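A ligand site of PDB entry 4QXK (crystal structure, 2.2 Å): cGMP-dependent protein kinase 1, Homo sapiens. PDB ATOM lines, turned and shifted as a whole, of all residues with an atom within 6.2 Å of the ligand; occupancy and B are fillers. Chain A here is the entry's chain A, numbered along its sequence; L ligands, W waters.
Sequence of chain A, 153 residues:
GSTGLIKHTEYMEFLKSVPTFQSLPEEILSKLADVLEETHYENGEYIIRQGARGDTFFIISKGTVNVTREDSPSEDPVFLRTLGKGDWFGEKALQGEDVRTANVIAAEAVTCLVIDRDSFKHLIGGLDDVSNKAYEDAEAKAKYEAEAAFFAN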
ATOM      1  N   ILE A  48       6.777 -22.609 -18.362  1.00  0.00           N
ATOM      2  CA  ILE A  48       5.620 -22.870 -19.195  1.00  0.00           C
ATOM      3  C   ILE A  48       5.952 -22.454 -20.624  1.00  0.00           C
ATOM      4  O   ILE A  48       6.507 -21.384 -20.847  1.00  0.00           O
ATOM      5  CB  ILE A  48       4.384 -22.022 -18.746  1.00  0.00           C
ATOM      6  CG1 ILE A  48       3.804 -22.554 -17.433  1.00  0.00           C
ATOM      7  CG2 ILE A  48       3.308 -22.007 -19.857  1.00  0.00           C
ATOM      8  CD1 ILE A  48       2.639 -21.728 -16.885  1.00  0.00           C
ATOM      9  N   THR A  56      -1.914 -27.082 -14.392  1.00  0.00           N
ATOM     10  CA  THR A  56      -1.311 -26.548 -13.155  1.00  0.00           C
ATOM     11  C   THR A  56      -1.288 -25.022 -13.032  1.00  0.00           C
ATOM     12  O   THR A  56      -1.059 -24.306 -14.021  1.00  0.00           O
ATOM     13  CB  THR A  56       0.119 -27.103 -12.979  1.00  0.00           C
ATOM     14  OG1 THR A  56       0.877 -26.930 -14.185  1.00  0.00           O
ATOM     15  CG2 THR A  56       0.159 -28.609 -12.623  1.00  0.00           C
ATOM     16  N   VAL A  67       7.583 -13.203 -18.967  1.00  0.00           N
ATOM     17  CA  VAL A  67       6.487 -13.725 -19.763  1.00  0.00           C
ATOM     18  C   VAL A  67       6.570 -13.160 -21.182  1.00  0.00           C
ATOM     19  O   VAL A  67       6.562 -11.949 -21.371  1.00  0.00           O
ATOM     20  CB  VAL A  67       5.114 -13.393 -19.142  1.00  0.00           C
ATOM     21  CG1 VAL A  67       3.979 -13.964 -19.995  1.00  0.00           C
ATOM     22  CG2 VAL A  67       5.035 -13.922 -17.700  1.00  0.00           C
ATOM     23  N   ARG A  69       5.183 -13.958 -25.469  1.00  0.00           N
ATOM     24  CA  ARG A  69       4.090 -14.570 -26.194  1.00  0.00           C
ATOM     25  C   ARG A  69       4.156 -14.283 -27.672  1.00  0.00           C
ATOM     26  O   ARG A  69       4.163 -13.122 -28.075  1.00  0.00           O
ATOM     27  CB  ARG A  69       2.769 -14.016 -25.641  1.00  0.00           C
ATOM     28  CG  ARG A  69       1.524 -14.428 -26.405  1.00  0.00           C
ATOM     29  CD  ARG A  69       0.271 -13.794 -25.798  1.00  0.00           C
ATOM     30  NE  ARG A  69      -0.932 -14.577 -26.067  1.00  0.00           N
ATOM     31  CZ  ARG A  69      -1.313 -14.963 -27.279  1.00  0.00           C
ATOM     32  NH1 ARG A  69      -0.635 -14.557 -28.342  1.00  0.00           N
ATOM     33  NH2 ARG A  69      -2.367 -15.759 -27.416  1.00  0.00           N
ATOM     34  N   LEU A  80       6.250  -9.687 -22.646  1.00  0.00           N
ATOM     35  CA  LEU A  80       4.992  -9.233 -22.057  1.00  0.00           C
ATOM     36  C   LEU A  80       5.105  -8.538 -20.702  1.00  0.00           C
ATOM     37  O   LEU A  80       4.665  -7.393 -20.548  1.00  0.00           O
ATOM     38  CB  LEU A  80       4.030 -10.418 -21.957  1.00  0.00           C
ATOM     39  CG  LEU A  80       2.865 -10.490 -22.952  1.00  0.00           C
ATOM     40  CD1 LEU A  80       3.271 -10.130 -24.370  1.00  0.00           C
ATOM     41  CD2 LEU A  80       2.326 -11.913 -22.907  1.00  0.00           C
ATOM     42  N   ARG A  81       5.689  -9.214 -19.709  1.00  0.00           N
ATOM     43  CA  ARG A  81       5.822  -8.618 -18.387  1.00  0.00           C
ATOM     44  C   ARG A  81       6.669  -9.485 -17.482  1.00  0.00           C
ATOM     45  O   ARG A  81       7.027 -10.607 -17.825  1.00  0.00           O
ATOM     46  CB  ARG A  81       4.452  -8.373 -17.748  1.00  0.00           C
ATOM     47  CG  ARG A  81       3.849  -9.591 -17.058  1.00  0.00           C
ATOM     48  CD  ARG A  81       2.411  -9.312 -16.651  1.00  0.00           C
ATOM     49  NE  ARG A  81       1.566  -9.083 -17.826  1.00  0.00           N
ATOM     50  CZ  ARG A  81       0.888  -7.969 -18.044  1.00  0.00           C
ATOM     51  NH1 ARG A  81       0.803  -7.047 -17.086  1.00  0.00           N
ATOM     52  NH2 ARG A  81       0.291  -7.762 -19.207  1.00  0.00           N
ATOM     53  N   LEU A  83       7.012 -11.038 -13.529  1.00  0.00           N
ATOM     54  CA  LEU A  83       6.256 -11.347 -12.326  1.00  0.00           C
ATOM     55  C   LEU A  83       7.258 -11.720 -11.240  1.00  0.00           C
ATOM     56  O   LEU A  83       8.306 -12.320 -11.523  1.00  0.00           O
ATOM     57  CB  LEU A  83       5.253 -12.482 -12.587  1.00  0.00           C
ATOM     58  CG  LEU A  83       4.182 -12.216 -13.640  1.00  0.00           C
ATOM     59  CD1 LEU A  83       3.303 -13.457 -13.782  1.00  0.00           C
ATOM     60  CD2 LEU A  83       3.322 -11.006 -13.255  1.00  0.00           C
ATOM     61  N   TRP A  88       1.178 -14.719  -9.342  1.00  0.00           N
ATOM     62  CA  TRP A  88       0.814 -16.064  -9.722  1.00  0.00           C
ATOM     63  C   TRP A  88       0.534 -16.096 -11.202  1.00  0.00           C
ATOM     64  O   TRP A  88       0.295 -15.064 -11.818  1.00  0.00           O
ATOM     65  CB  TRP A  88      -0.384 -16.575  -8.905  1.00  0.00           C
ATOM     66  CG  TRP A  88      -1.471 -15.570  -8.658  1.00  0.00           C
ATOM     67  CD1 TRP A  88      -1.718 -14.898  -7.493  1.00  0.00           C
ATOM     68  CD2 TRP A  88      -2.468 -15.116  -9.594  1.00  0.00           C
ATOM     69  NE1 TRP A  88      -2.810 -14.081  -7.640  1.00  0.00           N
ATOM     70  CE2 TRP A  88      -3.280 -14.185  -8.921  1.00  0.00           C
ATOM     71  CE3 TRP A  88      -2.736 -15.411 -10.939  1.00  0.00           C
ATOM     72  CZ2 TRP A  88      -4.357 -13.545  -9.545  1.00  0.00           C
ATOM     73  CZ3 TRP A  88      -3.794 -14.777 -11.549  1.00  0.00           C
ATOM     74  CH2 TRP A  88      -4.595 -13.851 -10.850  1.00  0.00           C
ATOM     75  N   PHE A  89       0.591 -17.299 -11.771  1.00  0.00           N
ATOM     76  CA  PHE A  89       0.345 -17.459 -13.194  1.00  0.00           C
ATOM     77  C   PHE A  89      -0.157 -18.871 -13.496  1.00  0.00           C
ATOM     78  O   PHE A  89      -0.185 -19.735 -12.616  1.00  0.00           O
ATOM     79  CB  PHE A  89       1.617 -17.132 -14.022  1.00  0.00           C
ATOM     80  CG  PHE A  89       2.835 -17.963 -13.679  1.00  0.00           C
ATOM     81  CD1 PHE A  89       3.725 -17.567 -12.699  1.00  0.00           C
ATOM     82  CD2 PHE A  89       3.092 -19.141 -14.361  1.00  0.00           C
ATOM     83  CE1 PHE A  89       4.831 -18.330 -12.396  1.00  0.00           C
ATOM     84  CE2 PHE A  89       4.193 -19.901 -14.071  1.00  0.00           C
ATOM     85  CZ  PHE A  89       5.066 -19.508 -13.086  1.00  0.00           C
ATOM     86  N   GLY A  90      -0.522 -19.087 -14.752  1.00  0.00           N
ATOM     87  CA  GLY A  90      -0.993 -20.374 -15.224  1.00  0.00           C
ATOM     88  C   GLY A  90      -2.492 -20.596 -15.131  1.00  0.00           C
ATOM     89  O   GLY A  90      -2.969 -21.696 -15.368  1.00  0.00           O
ATOM     90  N   GLU A  91      -3.241 -19.552 -14.799  1.00  0.00           N
ATOM     91  CA  GLU A  91      -4.682 -19.688 -14.676  1.00  0.00           C
ATOM     92  C   GLU A  91      -5.433 -19.838 -15.988  1.00  0.00           C
ATOM     93  O   GLU A  91      -6.514 -20.432 -15.995  1.00  0.00           O
ATOM     94  CB  GLU A  91      -5.304 -18.531 -13.884  1.00  0.00           C
ATOM     95  CG  GLU A  91      -5.629 -17.232 -14.683  1.00  0.00           C
ATOM     96  CD  GLU A  91      -4.393 -16.452 -15.130  1.00  0.00           C
ATOM     97  OE1 GLU A  91      -3.274 -16.794 -14.731  1.00  0.00           O
ATOM     98  OE2 GLU A  91      -4.568 -15.464 -15.868  1.00  0.00           O
ATOM     99  N   LYS A  92      -4.906 -19.289 -17.073  1.00  0.00           N
ATOM    100  CA  LYS A  92      -5.621 -19.380 -18.347  1.00  0.00           C
ATOM    101  C   LYS A  92      -5.871 -20.804 -18.839  1.00  0.00           C
ATOM    102  O   LYS A  92      -6.975 -21.099 -19.248  1.00  0.00           O
ATOM    103  CB  LYS A  92      -5.008 -18.470 -19.442  1.00  0.00           C
ATOM    104  CG  LYS A  92      -5.087 -16.968 -19.104  1.00  0.00           C
ATOM    105  CD  LYS A  92      -6.537 -16.500 -18.958  1.00  0.00           C
ATOM    106  CE  LYS A  92      -6.680 -14.998 -18.696  1.00  0.00           C
ATOM    107  NZ  LYS A  92      -7.116 -14.699 -17.279  1.00  0.00           N
ATOM    108  N   ALA A  93      -4.887 -21.683 -18.741  1.00  0.00           N
ATOM    109  CA  ALA A  93      -5.097 -23.075 -19.148  1.00  0.00           C
ATOM    110  C   ALA A  93      -6.125 -23.778 -18.250  1.00  0.00           C
ATOM    111  O   ALA A  93      -6.543 -24.899 -18.532  1.00  0.00           O
ATOM    112  CB  ALA A  93      -3.780 -23.839 -19.093  1.00  0.00           C
ATOM    113  N   LEU A  94      -6.504 -23.119 -17.152  1.00  0.00           N
ATOM    114  CA  LEU A  94      -7.462 -23.699 -16.214  1.00  0.00           C
ATOM    115  C   LEU A  94      -8.881 -23.140 -16.355  1.00  0.00           C
ATOM    116  O   LEU A  94      -9.793 -23.538 -15.625  1.00  0.00           O
ATOM    117  CB  LEU A  94      -6.948 -23.539 -14.781  1.00  0.00           C
ATOM    118  CG  LEU A  94      -5.584 -24.221 -14.562  1.00  0.00           C
ATOM    119  CD1 LEU A  94      -5.134 -24.024 -13.142  1.00  0.00           C
ATOM    120  CD2 LEU A  94      -5.627 -25.705 -14.878  1.00  0.00           C
ATOM    121  N   VAL A  99      -5.099 -24.790 -23.109  1.00  0.00           N
ATOM    122  CA  VAL A  99      -3.854 -24.467 -23.780  1.00  0.00           C
ATOM    123  C   VAL A  99      -3.167 -23.250 -23.153  1.00  0.00           C
ATOM    124  O   VAL A  99      -3.823 -22.268 -22.796  1.00  0.00           O
ATOM    125  CB  VAL A  99      -4.069 -24.316 -25.319  1.00  0.00           C
ATOM    126  CG1 VAL A  99      -4.931 -23.122 -25.616  1.00  0.00           C
ATOM    127  CG2 VAL A  99      -2.744 -24.227 -26.062  1.00  0.00           C
ATOM    128  N   ARG A 100      -1.849 -23.326 -23.020  1.00  0.00           N
ATOM    129  CA  ARG A 100      -1.081 -22.236 -22.433  1.00  0.00           C
ATOM    130  C   ARG A 100      -0.985 -21.118 -23.475  1.00  0.00           C
ATOM    131  O   ARG A 100      -0.670 -21.363 -24.635  1.00  0.00           O
ATOM    132  CB  ARG A 100       0.317 -22.705 -22.028  1.00  0.00           C
ATOM    133  CG  ARG A 100       0.367 -23.808 -20.971  1.00  0.00           C
ATOM    134  CD  ARG A 100      -0.088 -23.336 -19.607  1.00  0.00           C
ATOM    135  NE  ARG A 100       0.259 -24.310 -18.575  1.00  0.00           N
ATOM    136  CZ  ARG A 100      -0.199 -24.289 -17.318  1.00  0.00           C
ATOM    137  NH1 ARG A 100      -1.010 -23.317 -16.947  1.00  0.00           N
ATOM    138  NH2 ARG A 100       0.158 -25.232 -16.438  1.00  0.00           N
ATOM    139  N   THR A 101      -1.297 -19.904 -23.058  1.00  0.00           N
ATOM    140  CA  THR A 101      -1.320 -18.745 -23.941  1.00  0.00           C
ATOM    141  C   THR A 101      -0.057 -17.910 -23.972  1.00  0.00           C
ATOM    142  O   THR A 101      -0.022 -16.872 -24.626  1.00  0.00           O
ATOM    143  CB  THR A 101      -2.516 -17.885 -23.568  1.00  0.00           C
ATOM    144  OG1 THR A 101      -2.286 -17.252 -22.321  1.00  0.00           O
ATOM    145  CG2 THR A 101      -3.808 -18.675 -23.459  1.00  0.00           C
ATOM    146  N   ALA A 102       0.978 -18.338 -23.256  1.00  0.00           N
ATOM    147  CA  ALA A 102       2.228 -17.597 -23.211  1.00  0.00           C
ATOM    148  C   ALA A 102       3.348 -18.442 -22.614  1.00  0.00           C
ATOM    149  O   ALA A 102       3.090 -19.431 -21.952  1.00  0.00           O
ATOM    150  CB  ALA A 102       2.043 -16.333 -22.381  1.00  0.00           C
ATOM    151  N   ASN A 103       4.597 -18.008 -22.822  1.00  0.00           N
ATOM    152  CA  ASN A 103       5.750 -18.695 -22.246  1.00  0.00           C
ATOM    153  C   ASN A 103       6.072 -17.981 -20.908  1.00  0.00           C
ATOM    154  O   ASN A 103       5.897 -16.764 -20.788  1.00  0.00           O
ATOM    155  CB  ASN A 103       6.988 -18.597 -23.163  1.00  0.00           C
ATOM    156  CG  ASN A 103       6.736 -19.078 -24.582  1.00  0.00           C
ATOM    157  OD1 ASN A 103       6.658 -20.276 -24.862  1.00  0.00           O
ATOM    158  ND2 ASN A 103       6.617 -18.134 -25.502  1.00  0.00           N
ATOM    159  N   VAL A 104       6.595 -18.719 -19.937  1.00  0.00           N
ATOM    160  CA  VAL A 104       7.000 -18.135 -18.655  1.00  0.00           C
ATOM    161  C   VAL A 104       8.361 -18.759 -18.382  1.00  0.00           C
ATOM    162  O   VAL A 104       8.464 -19.969 -18.191  1.00  0.00           O
ATOM    163  CB  VAL A 104       6.005 -18.445 -17.513  1.00  0.00           C
ATOM    164  CG1 VAL A 104       6.357 -17.636 -16.273  1.00  0.00           C
ATOM    165  CG2 VAL A 104       4.596 -18.123 -17.949  1.00  0.00           C
ATOM    166  N   TYR A 135      -5.468  -8.993 -18.494  1.00  0.00           N
ATOM    167  CA  TYR A 135      -4.160  -8.399 -18.758  1.00  0.00           C
ATOM    168  C   TYR A 135      -4.206  -7.245 -19.765  1.00  0.00           C
ATOM    169  O   TYR A 135      -4.118  -6.082 -19.318  1.00  0.00           O
ATOM    170  CB  TYR A 135      -3.197  -9.484 -19.248  1.00  0.00           C
ATOM    171  CG  TYR A 135      -3.116 -10.650 -18.312  1.00  0.00           C
ATOM    172  CD1 TYR A 135      -4.108 -11.626 -18.290  1.00  0.00           C
ATOM    173  CD2 TYR A 135      -2.070 -10.770 -17.425  1.00  0.00           C
ATOM    174  CE1 TYR A 135      -4.043 -12.679 -17.407  1.00  0.00           C
ATOM    175  CE2 TYR A 135      -1.995 -11.813 -16.543  1.00  0.00           C
ATOM    176  CZ  TYR A 135      -2.981 -12.769 -16.542  1.00  0.00           C
ATOM    177  OH  TYR A 135      -2.913 -13.802 -15.639  1.00  0.00           O
HETATM  178  P1  LIG L   1      -1.476 -19.668 -18.911  1.00  0.00           P
HETATM  179  O1  LIG L   1      -2.201 -20.838 -18.341  1.00  0.00           O
HETATM  180  O2  LIG L   1      -1.901 -19.200 -20.353  1.00  0.00           O
HETATM  181  O3  LIG L   1       0.030 -19.953 -18.864  1.00  0.00           O
HETATM  182  C1  LIG L   1       0.860 -18.778 -19.327  1.00  0.00           C
HETATM  183  C2  LIG L   1       0.611 -17.676 -18.346  1.00  0.00           C
HETATM  184  O4  LIG L   1       1.221 -16.424 -18.547  1.00  0.00           O
HETATM  185  C3  LIG L   1      -0.848 -17.319 -18.239  1.00  0.00           C
HETATM  186  O5  LIG L   1      -1.705 -18.446 -17.894  1.00  0.00           O
HETATM  187  C4  LIG L   1      -0.897 -16.172 -17.280  1.00  0.00           C
HETATM  188  O6  LIG L   1      -1.197 -16.537 -15.976  1.00  0.00           O
HETATM  189  C5  LIG L   1       0.556 -15.602 -17.522  1.00  0.00           C
HETATM  190  N1  LIG L   1       0.558 -14.238 -18.029  1.00  0.00           N
HETATM  191  C6  LIG L   1       1.154 -13.088 -17.367  1.00  0.00           C
HETATM  192  N2  LIG L   1       0.903 -11.970 -18.231  1.00  0.00           N
HETATM  193  C7  LIG L   1       0.179 -12.416 -19.406  1.00  0.00           C
HETATM  194  C8  LIG L   1      -0.339 -11.721 -20.616  1.00  0.00           C
HETATM  195  O7  LIG L   1      -0.154 -10.354 -20.767  1.00  0.00           O
HETATM  196  N3  LIG L   1      -0.990 -12.420 -21.601  1.00  0.00           N
HETATM  197  C9  LIG L   1      -1.181 -13.830 -21.465  1.00  0.00           C
HETATM  198  N4  LIG L   1      -1.868 -14.597 -22.498  1.00  0.00           N
HETATM  199  N5  LIG L   1      -0.687 -14.542 -20.266  1.00  0.00           N
HETATM  200  C10 LIG L   1      -0.029 -13.813 -19.292  1.00  0.00           C
HETATM  201  O   HOH W   1      -1.541 -12.336 -24.146  1.00  0.00           O
HETATM  202  O   HOH W   2      -0.127 -13.779 -14.321  1.00  0.00           O
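O6 of the ligand sits at hydrogen-bond distance from N of Gly 90 (2.9 Å). The side-chain hydroxyl of Tyr 135 sits at hydrogen-bond distance from an oxygen (O6) of the ligand, 3.2 Å away. N of Thr 101 lies within hydrogen-bond range of O2 of the ligand, 2.9 Å away. The guanidinium group (NH1) of Arg 100 is in salt-bridge range of an oxygen (O1) of the ligand (3.1 Å). The side-chain hydroxyl of Thr 101 lies within hydrogen-bond range of a nitrogen (N4) of the ligand, at 2.7 Å. NE of Arg 81 lies within hydrogen-bond range of N2 of the ligand (3.0 Å). An oxygen (O1) of the ligand is in hydrogen-bond range of the backbone NH of Lys 92, 3.4 Å away. The side-chain carboxylate of Glu 91 is in hydrogen-bond range of an oxygen (O6) of the ligand (2.4 Å). The backbone NH (N) of Ala 93 is in hydrogen-bond range of an oxygen (O1) of the ligand.
O of Ile 48 sits at hydrogen-bond distance from N of Val 104, at 2.8 Å. NH1 of Arg 100 sits at hydrogen-bond distance from O of Gly 90 (3.0 Å). The backbone carbonyl oxygen (O) of Val 67 lies within hydrogen-bond range of the backbone NH (N) of Leu 80 (2.6 Å). OE2 of Glu 91 is in salt-bridge range of NZ of Lys 92, at 3.0 Å. O of Thr 101 lies within hydrogen-bond range of NE of Arg 69 (2.9 Å). The side-chain carboxylate (OE1) of Glu 91 sits close to the side-chain hydroxyl (OH) of Tyr 135 (3.1 Å). O of Arg 81 lies within hydrogen-bond range of N of Val 67 (2.9 Å). The guanidinium group (NH2) of Arg 100 lies within hydrogen-bond range of the backbone carbonyl oxygen (O) of Thr 56 (2.9 Å).
Residues that only touch the ligand: Phe 89 (3.3 Å), Ala 102 (3.5 Å), Leu 80 (3.5 Å), Arg 69 (3.7 Å), Ile 48 (3.7 Å), Val 104 (3.8 Å) and Val 67 (3.96 Å). Hydrophobic or aromatic side chains that line the ligand: Ile 48, Val 67, Leu 80, Phe 89, Ala 93, Ala 102, Val 104 and Tyr 135. 15 residues have an atom within 4 Å of the ligand: Ile 48, Val 67, Arg 69, Leu 80, Arg 81, Phe 89, Gly 90, Glu 91, Lys 92, Ala 93, Arg 100, Thr 101, Ala 102, Val 104 and Tyr 135. Along chain A the residues within 4 Å of the ligand span positions 48 to 135. The nearest printed residue that does not touch the ligand is Leu 83 (4.2 Å).
Water W1 lies within hydrogen-bond range of N3 of the ligand and NE of Arg 69. Water W2 lies within hydrogen-bond range of O of Trp 88 (2.8 Å), OH of Tyr 135 (3.1 Å) and O6 of the ligand (3.4 Å).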
